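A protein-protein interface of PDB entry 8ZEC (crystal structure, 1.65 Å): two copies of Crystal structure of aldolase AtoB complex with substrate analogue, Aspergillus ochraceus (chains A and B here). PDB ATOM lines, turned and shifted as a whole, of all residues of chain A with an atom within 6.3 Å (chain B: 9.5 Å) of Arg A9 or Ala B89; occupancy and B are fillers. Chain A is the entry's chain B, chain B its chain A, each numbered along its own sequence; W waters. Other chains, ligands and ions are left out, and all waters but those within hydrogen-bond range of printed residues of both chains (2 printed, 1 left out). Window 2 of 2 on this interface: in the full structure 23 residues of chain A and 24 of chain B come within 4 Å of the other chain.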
ATOM      1  N   LEU A   6      -3.189 -16.745 -21.366  1.00  0.00           N
ATOM      2  CA  LEU A   6      -4.365 -16.472 -22.192  1.00  0.00           C
ATOM      3  C   LEU A   6      -5.593 -17.150 -21.616  1.00  0.00           C
ATOM      4  O   LEU A   6      -5.502 -18.290 -21.179  1.00  0.00           O
ATOM      5  CB  LEU A   6      -4.192 -17.029 -23.602  1.00  0.00           C
ATOM      6  CG  LEU A   6      -3.015 -16.477 -24.382  1.00  0.00           C
ATOM      7  CD1 LEU A   6      -2.891 -17.174 -25.729  1.00  0.00           C
ATOM      8  CD2 LEU A   6      -3.134 -14.952 -24.511  1.00  0.00           C
ATOM      9  N   PRO A   7      -6.788 -16.517 -21.692  1.00  0.00           N
ATOM     10  CA  PRO A   7      -8.017 -17.191 -21.287  1.00  0.00           C
ATOM     11  C   PRO A   7      -8.147 -18.510 -22.067  1.00  0.00           C
ATOM     12  O   PRO A   7      -7.694 -18.625 -23.219  1.00  0.00           O
ATOM     13  CB  PRO A   7      -9.116 -16.182 -21.646  1.00  0.00           C
ATOM     14  CG  PRO A   7      -8.420 -14.838 -21.550  1.00  0.00           C
ATOM     15  CD  PRO A   7      -7.012 -15.105 -22.077  1.00  0.00           C
ATOM     16  N   LEU A   8      -8.762 -19.513 -21.432  1.00  0.00           N
ATOM     17  CA  LEU A   8      -8.764 -20.853 -21.986  1.00  0.00           C
ATOM     18  C   LEU A   8      -9.385 -20.908 -23.383  1.00  0.00           C
ATOM     19  O   LEU A   8      -8.833 -21.570 -24.246  1.00  0.00           O
ATOM     20  CB  LEU A   8      -9.490 -21.804 -21.040  1.00  0.00           C
ATOM     21  CG  LEU A   8      -9.616 -23.237 -21.555  1.00  0.00           C
ATOM     22  CD1 LEU A   8      -8.241 -23.904 -21.737  1.00  0.00           C
ATOM     23  CD2 LEU A   8     -10.485 -24.082 -20.624  1.00  0.00           C
ATOM     24  N   ARG A   9     -10.467 -20.143 -23.659  1.00  0.00           N
ATOM     25  CA  ARG A   9     -11.077 -20.192 -24.967  1.00  0.00           C
ATOM     26  C   ARG A   9     -10.046 -19.851 -26.041  1.00  0.00           C
ATOM     27  O   ARG A   9     -10.020 -20.489 -27.087  1.00  0.00           O
ATOM     28  CB  ARG A   9     -12.366 -19.386 -24.988  1.00  0.00           C
ATOM     29  CG  ARG A   9     -13.148 -19.490 -26.275  1.00  0.00           C
ATOM     30  CD  ARG A   9     -14.376 -18.625 -26.240  1.00  0.00           C
ATOM     31  NE  ARG A   9     -15.261 -18.782 -27.354  1.00  0.00           N
ATOM     32  CZ  ARG A   9     -16.260 -19.663 -27.434  1.00  0.00           C
ATOM     33  NH1 ARG A   9     -16.790 -20.205 -26.353  1.00  0.00           N
ATOM     34  NH2 ARG A   9     -16.787 -19.900 -28.618  1.00  0.00           N
ATOM     35  N   GLU A  10      -9.365 -18.736 -25.865  1.00  0.00           N
ATOM     36  CA  GLU A  10      -8.402 -18.226 -26.809  1.00  0.00           C
ATOM     37  C   GLU A  10      -7.230 -19.200 -26.964  1.00  0.00           C
ATOM     38  O   GLU A  10      -6.762 -19.410 -28.075  1.00  0.00           O
ATOM     39  CB  GLU A  10      -7.922 -16.860 -26.307  1.00  0.00           C
ATOM     40  CG  GLU A  10      -6.784 -16.299 -27.114  1.00  0.00           C
ATOM     41  CD  GLU A  10      -6.342 -14.909 -26.712  1.00  0.00           C
ATOM     42  OE1 GLU A  10      -6.662 -14.523 -25.600  1.00  0.00           O
ATOM     43  OE2 GLU A  10      -5.724 -14.241 -27.532  1.00  0.00           O
ATOM     44  N   ARG A  11      -6.759 -19.752 -25.843  1.00  0.00           N
ATOM     45  CA  ARG A  11      -5.699 -20.727 -25.819  1.00  0.00           C
ATOM     46  C   ARG A  11      -6.077 -21.913 -26.740  1.00  0.00           C
ATOM     47  O   ARG A  11      -5.263 -22.404 -27.516  1.00  0.00           O
ATOM     48  CB  ARG A  11      -5.461 -21.162 -24.369  1.00  0.00           C
ATOM     49  CG  ARG A  11      -4.097 -21.779 -24.126  1.00  0.00           C
ATOM     50  CD  ARG A  11      -3.675 -21.606 -22.662  1.00  0.00           C
ATOM     51  NE  ARG A  11      -4.362 -22.466 -21.777  1.00  0.00           N
ATOM     52  CZ  ARG A  11      -4.978 -22.104 -20.668  1.00  0.00           C
ATOM     53  NH1 ARG A  11      -5.287 -20.855 -20.426  1.00  0.00           N
ATOM     54  NH2 ARG A  11      -5.483 -23.058 -19.921  1.00  0.00           N
ATOM     55  N   LEU A  12      -7.299 -22.409 -26.593  1.00  0.00           N
ATOM     56  CA  LEU A  12      -7.768 -23.599 -27.307  1.00  0.00           C
ATOM     57  C   LEU A  12      -7.822 -23.304 -28.811  1.00  0.00           C
ATOM     58  O   LEU A  12      -7.378 -24.067 -29.645  1.00  0.00           O
ATOM     59  CB  LEU A  12      -9.136 -24.032 -26.797  1.00  0.00           C
ATOM     60  CG  LEU A  12      -9.218 -24.645 -25.405  1.00  0.00           C
ATOM     61  CD1 LEU A  12     -10.673 -24.824 -24.996  1.00  0.00           C
ATOM     62  CD2 LEU A  12      -8.473 -25.982 -25.332  1.00  0.00           C
ATOM     63  N   ILE A  13      -8.295 -22.132 -29.178  1.00  0.00           N
ATOM     64  CA  ILE A  13      -8.403 -21.786 -30.589  1.00  0.00           C
ATOM     65  C   ILE A  13      -6.997 -21.675 -31.165  1.00  0.00           C
ATOM     66  O   ILE A  13      -6.745 -22.188 -32.235  1.00  0.00           O
ATOM     67  CB  ILE A  13      -9.193 -20.481 -30.808  1.00  0.00           C
ATOM     68  CG1 ILE A  13     -10.664 -20.658 -30.454  1.00  0.00           C
ATOM     69  CG2 ILE A  13      -9.019 -19.933 -32.221  1.00  0.00           C
ATOM     70  CD1 ILE A  13     -11.391 -19.421 -30.191  1.00  0.00           C
ATOM     71  N   GLN A  14      -6.063 -21.042 -30.431  1.00  0.00           N
ATOM     72  CA  GLN A  14      -4.695 -20.898 -30.917  1.00  0.00           C
ATOM     73  C   GLN A  14      -4.001 -22.265 -31.078  1.00  0.00           C
ATOM     74  O   GLN A  14      -3.367 -22.537 -32.067  1.00  0.00           O
ATOM     75  CB  GLN A  14      -3.874 -20.035 -29.991  1.00  0.00           C
ATOM     76  CG  GLN A  14      -2.487 -19.674 -30.489  1.00  0.00           C
ATOM     77  CD  GLN A  14      -1.905 -18.514 -29.682  1.00  0.00           C
ATOM     78  OE1 GLN A  14      -2.602 -17.568 -29.292  1.00  0.00           O
ATOM     79  NE2 GLN A  14      -0.642 -18.609 -29.324  1.00  0.00           N
ATOM     80  N   PRO A  84     -15.216 -20.956 -35.341  1.00  0.00           N
ATOM     81  CA  PRO A  84     -14.729 -21.972 -34.419  1.00  0.00           C
ATOM     82  C   PRO A  84     -15.727 -22.271 -33.296  1.00  0.00           C
ATOM     83  O   PRO A  84     -16.323 -21.363 -32.713  1.00  0.00           O
ATOM     84  CB  PRO A  84     -13.446 -21.366 -33.840  1.00  0.00           C
ATOM     85  CG  PRO A  84     -13.230 -20.068 -34.555  1.00  0.00           C
ATOM     86  CD  PRO A  84     -14.588 -19.654 -35.092  1.00  0.00           C
ATOM     87  N   ILE A  85     -15.999 -23.560 -33.078  1.00  0.00           N
ATOM     88  CA  ILE A  85     -16.882 -24.072 -32.046  1.00  0.00           C
ATOM     89  C   ILE A  85     -16.007 -24.612 -30.918  1.00  0.00           C
ATOM     90  O   ILE A  85     -15.242 -25.555 -31.070  1.00  0.00           O
ATOM     91  CB  ILE A  85     -17.830 -25.144 -32.610  1.00  0.00           C
ATOM     92  CG1 ILE A  85     -18.656 -24.562 -33.766  1.00  0.00           C
ATOM     93  CG2 ILE A  85     -18.665 -25.697 -31.478  1.00  0.00           C
ATOM     94  CD1 ILE A  85     -19.375 -25.586 -34.545  1.00  0.00           C
ATOM     95  N   VAL A  86     -16.098 -23.962 -29.775  1.00  0.00           N
ATOM     96  CA  VAL A  86     -15.193 -24.249 -28.679  1.00  0.00           C
ATOM     97  C   VAL A  86     -15.951 -24.745 -27.478  1.00  0.00           C
ATOM     98  O   VAL A  86     -16.808 -24.035 -26.951  1.00  0.00           O
ATOM     99  CB  VAL A  86     -14.382 -22.994 -28.276  1.00  0.00           C
ATOM    100  CG1 VAL A  86     -13.363 -23.407 -27.241  1.00  0.00           C
ATOM    101  CG2 VAL A  86     -13.790 -22.302 -29.461  1.00  0.00           C
ATOM    102  N   ASP A  87     -15.541 -25.928 -26.998  1.00  0.00           N
ATOM    103  CA  ASP A  87     -16.073 -26.506 -25.793  1.00  0.00           C
ATOM    104  C   ASP A  87     -14.961 -26.500 -24.749  1.00  0.00           C
ATOM    105  O   ASP A  87     -14.081 -27.403 -24.750  1.00  0.00           O
ATOM    106  CB  ASP A  87     -16.618 -27.908 -26.072  1.00  0.00           C
ATOM    107  CG  ASP A  87     -17.246 -28.551 -24.860  1.00  0.00           C
ATOM    108  OD1 ASP A  87     -17.025 -28.009 -23.701  1.00  0.00           O
ATOM    109  OD2 ASP A  87     -18.074 -29.497 -25.043  1.00  0.00           O
ATOM    110  N   GLU A  88     -14.950 -25.439 -23.928  1.00  0.00           N
ATOM    111  CA  GLU A  88     -13.882 -25.267 -22.940  1.00  0.00           C
ATOM    112  C   GLU A  88     -13.771 -26.500 -22.019  1.00  0.00           C
ATOM    113  O   GLU A  88     -12.660 -27.000 -21.791  1.00  0.00           O
ATOM    114  CB  GLU A  88     -14.066 -23.930 -22.201  1.00  0.00           C
ATOM    115  CG  GLU A  88     -13.933 -22.751 -23.114  1.00  0.00           C
ATOM    116  CD  GLU A  88     -14.339 -21.407 -22.533  1.00  0.00           C
ATOM    117  OE1 GLU A  88     -13.828 -21.077 -21.474  1.00  0.00           O
ATOM    118  OE2 GLU A  88     -15.177 -20.664 -23.184  1.00  0.00           O
ATOM    119  N   VAL A  93     -12.113 -28.103 -29.958  1.00  0.00           N
ATOM    120  CA  VAL A  93     -12.418 -27.100 -30.968  1.00  0.00           C
ATOM    121  C   VAL A  93     -12.855 -27.803 -32.252  1.00  0.00           C
ATOM    122  O   VAL A  93     -12.198 -28.729 -32.719  1.00  0.00           O
ATOM    123  CB  VAL A  93     -11.268 -26.092 -31.234  1.00  0.00           C
ATOM    124  CG1 VAL A  93     -11.602 -25.041 -32.284  1.00  0.00           C
ATOM    125  CG2 VAL A  93     -10.701 -25.478 -29.971  1.00  0.00           C
ATOM    126  N   LEU B   8     -27.681 -24.039 -19.153  1.00  0.00           N
ATOM    127  CA  LEU B   8     -27.625 -23.835 -20.587  1.00  0.00           C
ATOM    128  C   LEU B   8     -26.963 -25.047 -21.258  1.00  0.00           C
ATOM    129  O   LEU B   8     -27.435 -25.512 -22.292  1.00  0.00           O
ATOM    130  CB  LEU B   8     -26.875 -22.547 -20.933  1.00  0.00           C
ATOM    131  CG  LEU B   8     -26.728 -22.228 -22.430  1.00  0.00           C
ATOM    132  CD1 LEU B   8     -28.066 -22.167 -23.133  1.00  0.00           C
ATOM    133  CD2 LEU B   8     -25.962 -20.941 -22.711  1.00  0.00           C
ATOM    134  N   ARG B   9     -25.847 -25.546 -20.725  1.00  0.00           N
ATOM    135  CA  ARG B   9     -25.217 -26.692 -21.359  1.00  0.00           C
ATOM    136  C   ARG B   9     -26.194 -27.839 -21.601  1.00  0.00           C
ATOM    137  O   ARG B   9     -26.288 -28.388 -22.721  1.00  0.00           O
ATOM    138  CB  ARG B   9     -24.063 -27.179 -20.519  1.00  0.00           C
ATOM    139  CG  ARG B   9     -23.120 -28.059 -21.280  1.00  0.00           C
ATOM    140  CD  ARG B   9     -21.982 -28.418 -20.396  1.00  0.00           C
ATOM    141  NE  ARG B   9     -21.106 -29.258 -21.120  1.00  0.00           N
ATOM    142  CZ  ARG B   9     -20.133 -28.872 -21.929  1.00  0.00           C
ATOM    143  NH1 ARG B   9     -19.754 -27.616 -22.041  1.00  0.00           N
ATOM    144  NH2 ARG B   9     -19.444 -29.812 -22.522  1.00  0.00           N
ATOM    145  N   LEU B  12     -28.944 -27.037 -24.242  1.00  0.00           N
ATOM    146  CA  LEU B  12     -28.415 -27.147 -25.591  1.00  0.00           C
ATOM    147  C   LEU B  12     -28.350 -28.606 -26.039  1.00  0.00           C
ATOM    148  O   LEU B  12     -28.819 -28.960 -27.113  1.00  0.00           O
ATOM    149  CB  LEU B  12     -27.047 -26.483 -25.692  1.00  0.00           C
ATOM    150  CG  LEU B  12     -27.016 -24.965 -25.552  1.00  0.00           C
ATOM    151  CD1 LEU B  12     -25.602 -24.429 -25.564  1.00  0.00           C
ATOM    152  CD2 LEU B  12     -27.778 -24.402 -26.676  1.00  0.00           C
ATOM    153  N   VAL B  86     -20.091 -29.013 -26.893  1.00  0.00           N
ATOM    154  CA  VAL B  86     -21.026 -27.937 -26.607  1.00  0.00           C
ATOM    155  C   VAL B  86     -20.296 -26.606 -26.428  1.00  0.00           C
ATOM    156  O   VAL B  86     -19.473 -26.456 -25.511  1.00  0.00           O
ATOM    157  CB  VAL B  86     -21.887 -28.212 -25.368  1.00  0.00           C
ATOM    158  CG1 VAL B  86     -22.919 -27.117 -25.285  1.00  0.00           C
ATOM    159  CG2 VAL B  86     -22.570 -29.572 -25.411  1.00  0.00           C
ATOM    160  N   ASP B  87     -20.661 -25.618 -27.259  1.00  0.00           N
ATOM    161  CA  ASP B  87     -20.184 -24.235 -27.176  1.00  0.00           C
ATOM    162  C   ASP B  87     -21.329 -23.344 -26.721  1.00  0.00           C
ATOM    163  O   ASP B  87     -22.151 -22.959 -27.544  1.00  0.00           O
ATOM    164  CB  ASP B  87     -19.599 -23.730 -28.483  1.00  0.00           C
ATOM    165  CG  ASP B  87     -19.003 -22.328 -28.470  1.00  0.00           C
ATOM    166  OD1 ASP B  87     -19.313 -21.561 -27.506  1.00  0.00           O
ATOM    167  OD2 ASP B  87     -18.178 -22.011 -29.398  1.00  0.00           O
ATOM    168  N   GLU B  88     -21.405 -23.106 -25.417  1.00  0.00           N
ATOM    169  CA  GLU B  88     -22.549 -22.417 -24.837  1.00  0.00           C
ATOM    170  C   GLU B  88     -22.653 -21.044 -25.501  1.00  0.00           C
ATOM    171  O   GLU B  88     -23.738 -20.607 -25.872  1.00  0.00           O
ATOM    172  CB  GLU B  88     -22.415 -22.398 -23.319  1.00  0.00           C
ATOM    173  CG  GLU B  88     -22.588 -23.759 -22.684  1.00  0.00           C
ATOM    174  CD  GLU B  88     -21.991 -23.927 -21.298  1.00  0.00           C
ATOM    175  OE1 GLU B  88     -22.467 -23.245 -20.396  1.00  0.00           O
ATOM    176  OE2 GLU B  88     -21.036 -24.769 -21.128  1.00  0.00           O
ATOM    177  N   ALA B  89     -21.507 -20.323 -25.548  1.00  0.00           N
ATOM    178  CA  ALA B  89     -21.454 -18.936 -25.997  1.00  0.00           C
ATOM    179  C   ALA B  89     -22.079 -18.790 -27.390  1.00  0.00           C
ATOM    180  O   ALA B  89     -22.801 -17.826 -27.682  1.00  0.00           O
ATOM    181  CB  ALA B  89     -20.014 -18.495 -26.069  1.00  0.00           C
ATOM    182  N   ASN B  90     -21.771 -19.780 -28.257  1.00  0.00           N
ATOM    183  CA  ASN B  90     -22.203 -19.779 -29.645  1.00  0.00           C
ATOM    184  C   ASN B  90     -23.493 -20.586 -29.866  1.00  0.00           C
ATOM    185  O   ASN B  90     -23.993 -20.634 -30.995  1.00  0.00           O
ATOM    186  CB  ASN B  90     -21.100 -20.228 -30.602  1.00  0.00           C
ATOM    187  CG  ASN B  90     -19.998 -19.233 -30.863  1.00  0.00           C
ATOM    188  OD1 ASN B  90     -20.249 -18.031 -30.987  1.00  0.00           O
ATOM    189  ND2 ASN B  90     -18.773 -19.744 -30.989  1.00  0.00           N
ATOM    190  N   ARG B  91     -24.089 -21.124 -28.810  1.00  0.00           N
ATOM    191  CA  ARG B  91     -25.319 -21.903 -28.905  1.00  0.00           C
ATOM    192  C   ARG B  91     -25.187 -23.048 -29.900  1.00  0.00           C
ATOM    193  O   ARG B  91     -26.109 -23.367 -30.653  1.00  0.00           O
ATOM    194  CB  ARG B  91     -26.462 -20.980 -29.262  1.00  0.00           C
ATOM    195  CG  ARG B  91     -26.666 -19.830 -28.292  1.00  0.00           C
ATOM    196  CD  ARG B  91     -27.097 -20.150 -26.890  1.00  0.00           C
ATOM    197  NE  ARG B  91     -27.490 -19.028 -26.054  1.00  0.00           N
ATOM    198  CZ  ARG B  91     -26.702 -18.138 -25.438  1.00  0.00           C
ATOM    199  NH1 ARG B  91     -25.400 -18.352 -25.318  1.00  0.00           N
ATOM    200  NH2 ARG B  91     -27.259 -17.062 -24.867  1.00  0.00           N
ATOM    201  N   LYS B  92     -24.030 -23.729 -29.858  1.00  0.00           N
ATOM    202  CA  LYS B  92     -23.787 -24.848 -30.773  1.00  0.00           C
ATOM    203  C   LYS B  92     -23.476 -26.142 -30.050  1.00  0.00           C
ATOM    204  O   LYS B  92     -22.892 -26.177 -28.965  1.00  0.00           O
ATOM    205  CB  LYS B  92     -22.658 -24.513 -31.750  1.00  0.00           C
ATOM    206  CG  LYS B  92     -23.010 -23.328 -32.635  1.00  0.00           C
ATOM    207  CD  LYS B  92     -22.202 -22.991 -33.794  1.00  0.00           C
ATOM    208  CE  LYS B  92     -22.651 -21.678 -34.369  1.00  0.00           C
ATOM    209  NZ  LYS B  92     -23.427 -21.988 -35.553  1.00  0.00           N
ATOM    210  N   VAL B  93     -23.921 -27.220 -30.703  1.00  0.00           N
ATOM    211  CA  VAL B  93     -23.637 -28.572 -30.271  1.00  0.00           C
ATOM    212  C   VAL B  93     -23.209 -29.409 -31.481  1.00  0.00           C
ATOM    213  O   VAL B  93     -23.785 -29.318 -32.560  1.00  0.00           O
ATOM    214  CB  VAL B  93     -24.843 -29.262 -29.607  1.00  0.00           C
ATOM    215  CG1 VAL B  93     -24.488 -30.654 -29.103  1.00  0.00           C
ATOM    216  CG2 VAL B  93     -25.504 -28.447 -28.530  1.00  0.00           C
ATOM    217  N   THR B 117     -27.307 -25.527 -34.196  1.00  0.00           N
ATOM    218  CA  THR B 117     -27.343 -24.182 -33.615  1.00  0.00           C
ATOM    219  C   THR B 117     -28.745 -23.924 -33.071  1.00  0.00           C
ATOM    220  O   THR B 117     -29.715 -24.096 -33.788  1.00  0.00           O
ATOM    221  CB  THR B 117     -26.952 -23.116 -34.637  1.00  0.00           C
ATOM    222  OG1 THR B 117     -25.751 -23.463 -35.327  1.00  0.00           O
ATOM    223  CG2 THR B 117     -26.771 -21.759 -33.994  1.00  0.00           C
ATOM    224  N   THR B 118     -28.829 -23.425 -31.836  1.00  0.00           N
ATOM    225  CA  THR B 118     -30.112 -23.106 -31.253  1.00  0.00           C
ATOM    226  C   THR B 118     -30.353 -21.587 -31.344  1.00  0.00           C
ATOM    227  O   THR B 118     -29.475 -20.760 -31.625  1.00  0.00           O
ATOM    228  CB  THR B 118     -30.197 -23.577 -29.812  1.00  0.00           C
ATOM    229  OG1 THR B 118     -29.433 -22.723 -28.967  1.00  0.00           O
ATOM    230  CG2 THR B 118     -29.742 -25.021 -29.675  1.00  0.00           C
ATOM    231  N   ASN B 119     -31.594 -21.234 -31.063  1.00  0.00           N
ATOM    232  CA  ASN B 119     -31.955 -19.880 -30.751  1.00  0.00           C
ATOM    233  C   ASN B 119     -31.202 -19.417 -29.501  1.00  0.00           C
ATOM    234  O   ASN B 119     -30.593 -20.228 -28.771  1.00  0.00           O
ATOM    235  CB  ASN B 119     -33.490 -19.787 -30.686  1.00  0.00           C
ATOM    236  CG  ASN B 119     -34.171 -20.653 -29.646  1.00  0.00           C
ATOM    237  OD1 ASN B 119     -33.503 -21.323 -28.837  1.00  0.00           O
ATOM    238  ND2 ASN B 119     -35.487 -20.546 -29.557  1.00  0.00           N
ATOM    239  N   ASP B 120     -31.328 -18.133 -29.170  1.00  0.00           N
ATOM    240  CA  ASP B 120     -30.611 -17.564 -28.046  1.00  0.00           C
ATOM    241  C   ASP B 120     -31.006 -18.248 -26.734  1.00  0.00           C
ATOM    242  O   ASP B 120     -30.166 -18.452 -25.855  1.00  0.00           O
ATOM    243  CB  ASP B 120     -30.736 -16.043 -28.053  1.00  0.00           C
ATOM    244  CG  ASP B 120     -29.960 -15.423 -26.925  1.00  0.00           C
ATOM    245  OD1 ASP B 120     -28.749 -15.648 -26.874  1.00  0.00           O
ATOM    246  OD2 ASP B 120     -30.610 -14.743 -26.115  1.00  0.00           O
ATOM    247  N   LYS B 126     -32.309 -23.537 -34.876  1.00  0.00           N
ATOM    248  CA  LYS B 126     -32.426 -22.612 -35.994  1.00  0.00           C
ATOM    249  C   LYS B 126     -31.563 -23.053 -37.169  1.00  0.00           C
ATOM    250  O   LYS B 126     -31.732 -22.538 -38.273  1.00  0.00           O
ATOM    251  CB  LYS B 126     -32.080 -21.178 -35.590  1.00  0.00           C
ATOM    252  CG  LYS B 126     -30.644 -20.868 -35.203  1.00  0.00           C
ATOM    253  CD  LYS B 126     -30.537 -19.383 -34.760  1.00  0.00           C
ATOM    254  CE  LYS B 126     -29.135 -18.850 -34.600  1.00  0.00           C
ATOM    255  NZ  LYS B 126     -29.112 -17.356 -34.548  1.00  0.00           N
HETATM  256  O   HOH W   1     -17.522 -25.469 -21.530  1.00  0.00           O
HETATM  257  O   HOH W   2     -16.248 -18.755 -32.026  1.00  0.00           O
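Ala B89 touches Arg A9.
Pro A84 touches Asp B87 (O to OD2, 3.9 Å).
Ile A85 touches Asp B87.
Ile A85 touches Lys B92 (CG1 to CD, 3.9 Å).
Val B86 touches Val A86 (O to O, 3.9 Å).
The guanidinium group (NH2) of Arg B9 lies within salt-bridge range of the side-chain carboxylate (OD2) of Asp A87.
OD2 of Asp A87 sits at hydrogen-bond distance from N of Val B86 (2.8 Å).
The guanidinium group of Arg A9 is in salt-bridge range of the side-chain carboxylate of Asp B87 (2.6 Å).
OD2 of Asp B87 lies within hydrogen-bond range of N of Val A86.
ND2 of Asn B90 sits close to NH2 of Arg A9 (3.1 Å).
The side-chain amide nitrogen (ND2) of Asn B90 lies within hydrogen-bond range of the backbone carbonyl oxygen (O) of Pro A84 (3.4 Å).
Water W2 bridges the backbone carbonyl oxygen of Pro A84 (2.7 Å) and the side-chain amide nitrogen of Asn B90 (2.9 Å).
Water W1 lies within hydrogen-bond range of NH1 of Arg B9 and OD1 of Asp A87.
The side-chain carboxylate of Glu B88 lies within salt-bridge range of the guanidinium group of Arg B9 (3.3 Å).
OD1 of Asp B87 lies within hydrogen-bond range of N of Ala B89.
The side-chain carboxylate (OD2) of Asp B87 sits at hydrogen-bond distance from the side-chain amide nitrogen (ND2) of Asn B90 (2.8 Å).
The backbone NH (N) of Asp B87 sits at hydrogen-bond distance from the backbone carbonyl oxygen (O) of Lys B92.
OG1 of Thr B117 is in hydrogen-bond range of NZ of Lys B92, 2.8 Å away.
The guanidinium group (NH1) of Arg A9 is in salt-bridge range of the side-chain carboxylate (OE2) of Glu A88, 3.6 Å away.
No residue of chain B comes within 4 Å of Leu A8.
Of the printed residues of chain B, Ile A85 touches Asp B87 (3.6 Å) and Lys B92 (3.9 Å).
Of the printed residues of chain B, Asp A87 touches Arg B9 (2.9 Å) and Val B86 (2.8 Å).
Leu B12 touches none of the printed residues of chain A.
Printed residues of chain A within 4 Å of Asp B87: Arg A9 (2.6 Å), Pro A84 (3.9 Å), Ile A85 (3.6 Å) and Val A86 (2.9 Å).
Of the printed residues of chain A, Asn B90 touches Arg A9 (3.1 Å) and Pro A84 (3.4 Å).
Printed residues of chain A within 4 Å of Lys B92: Ile A85 (3.9 Å).
The nearest residue of chain A that does not touch Ala B89 is Glu A88 (6.0 Å).
Hydrophobic or aromatic side chains of chain A within 4 Å of the printed part of chain B: Ile A85.
Of the 16 printed residues of chain B, 6 touch a printed residue of chain A.
Arg A9 touches Asp B87, and with the chains exchanged Asp A87 touches Arg B9.
Val B86 touches its own counterpart, Val A86.
Val A86 touches Asp B87, and with the chains exchanged Asp A87 touches Val B86.
Positions printed for both chains: 8, 9, 12, 86, 87, 88 and 93.
Of the 11 pairs that touch across the chains among the printed residues, 5 have their exchanged pair printed and touching as well.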
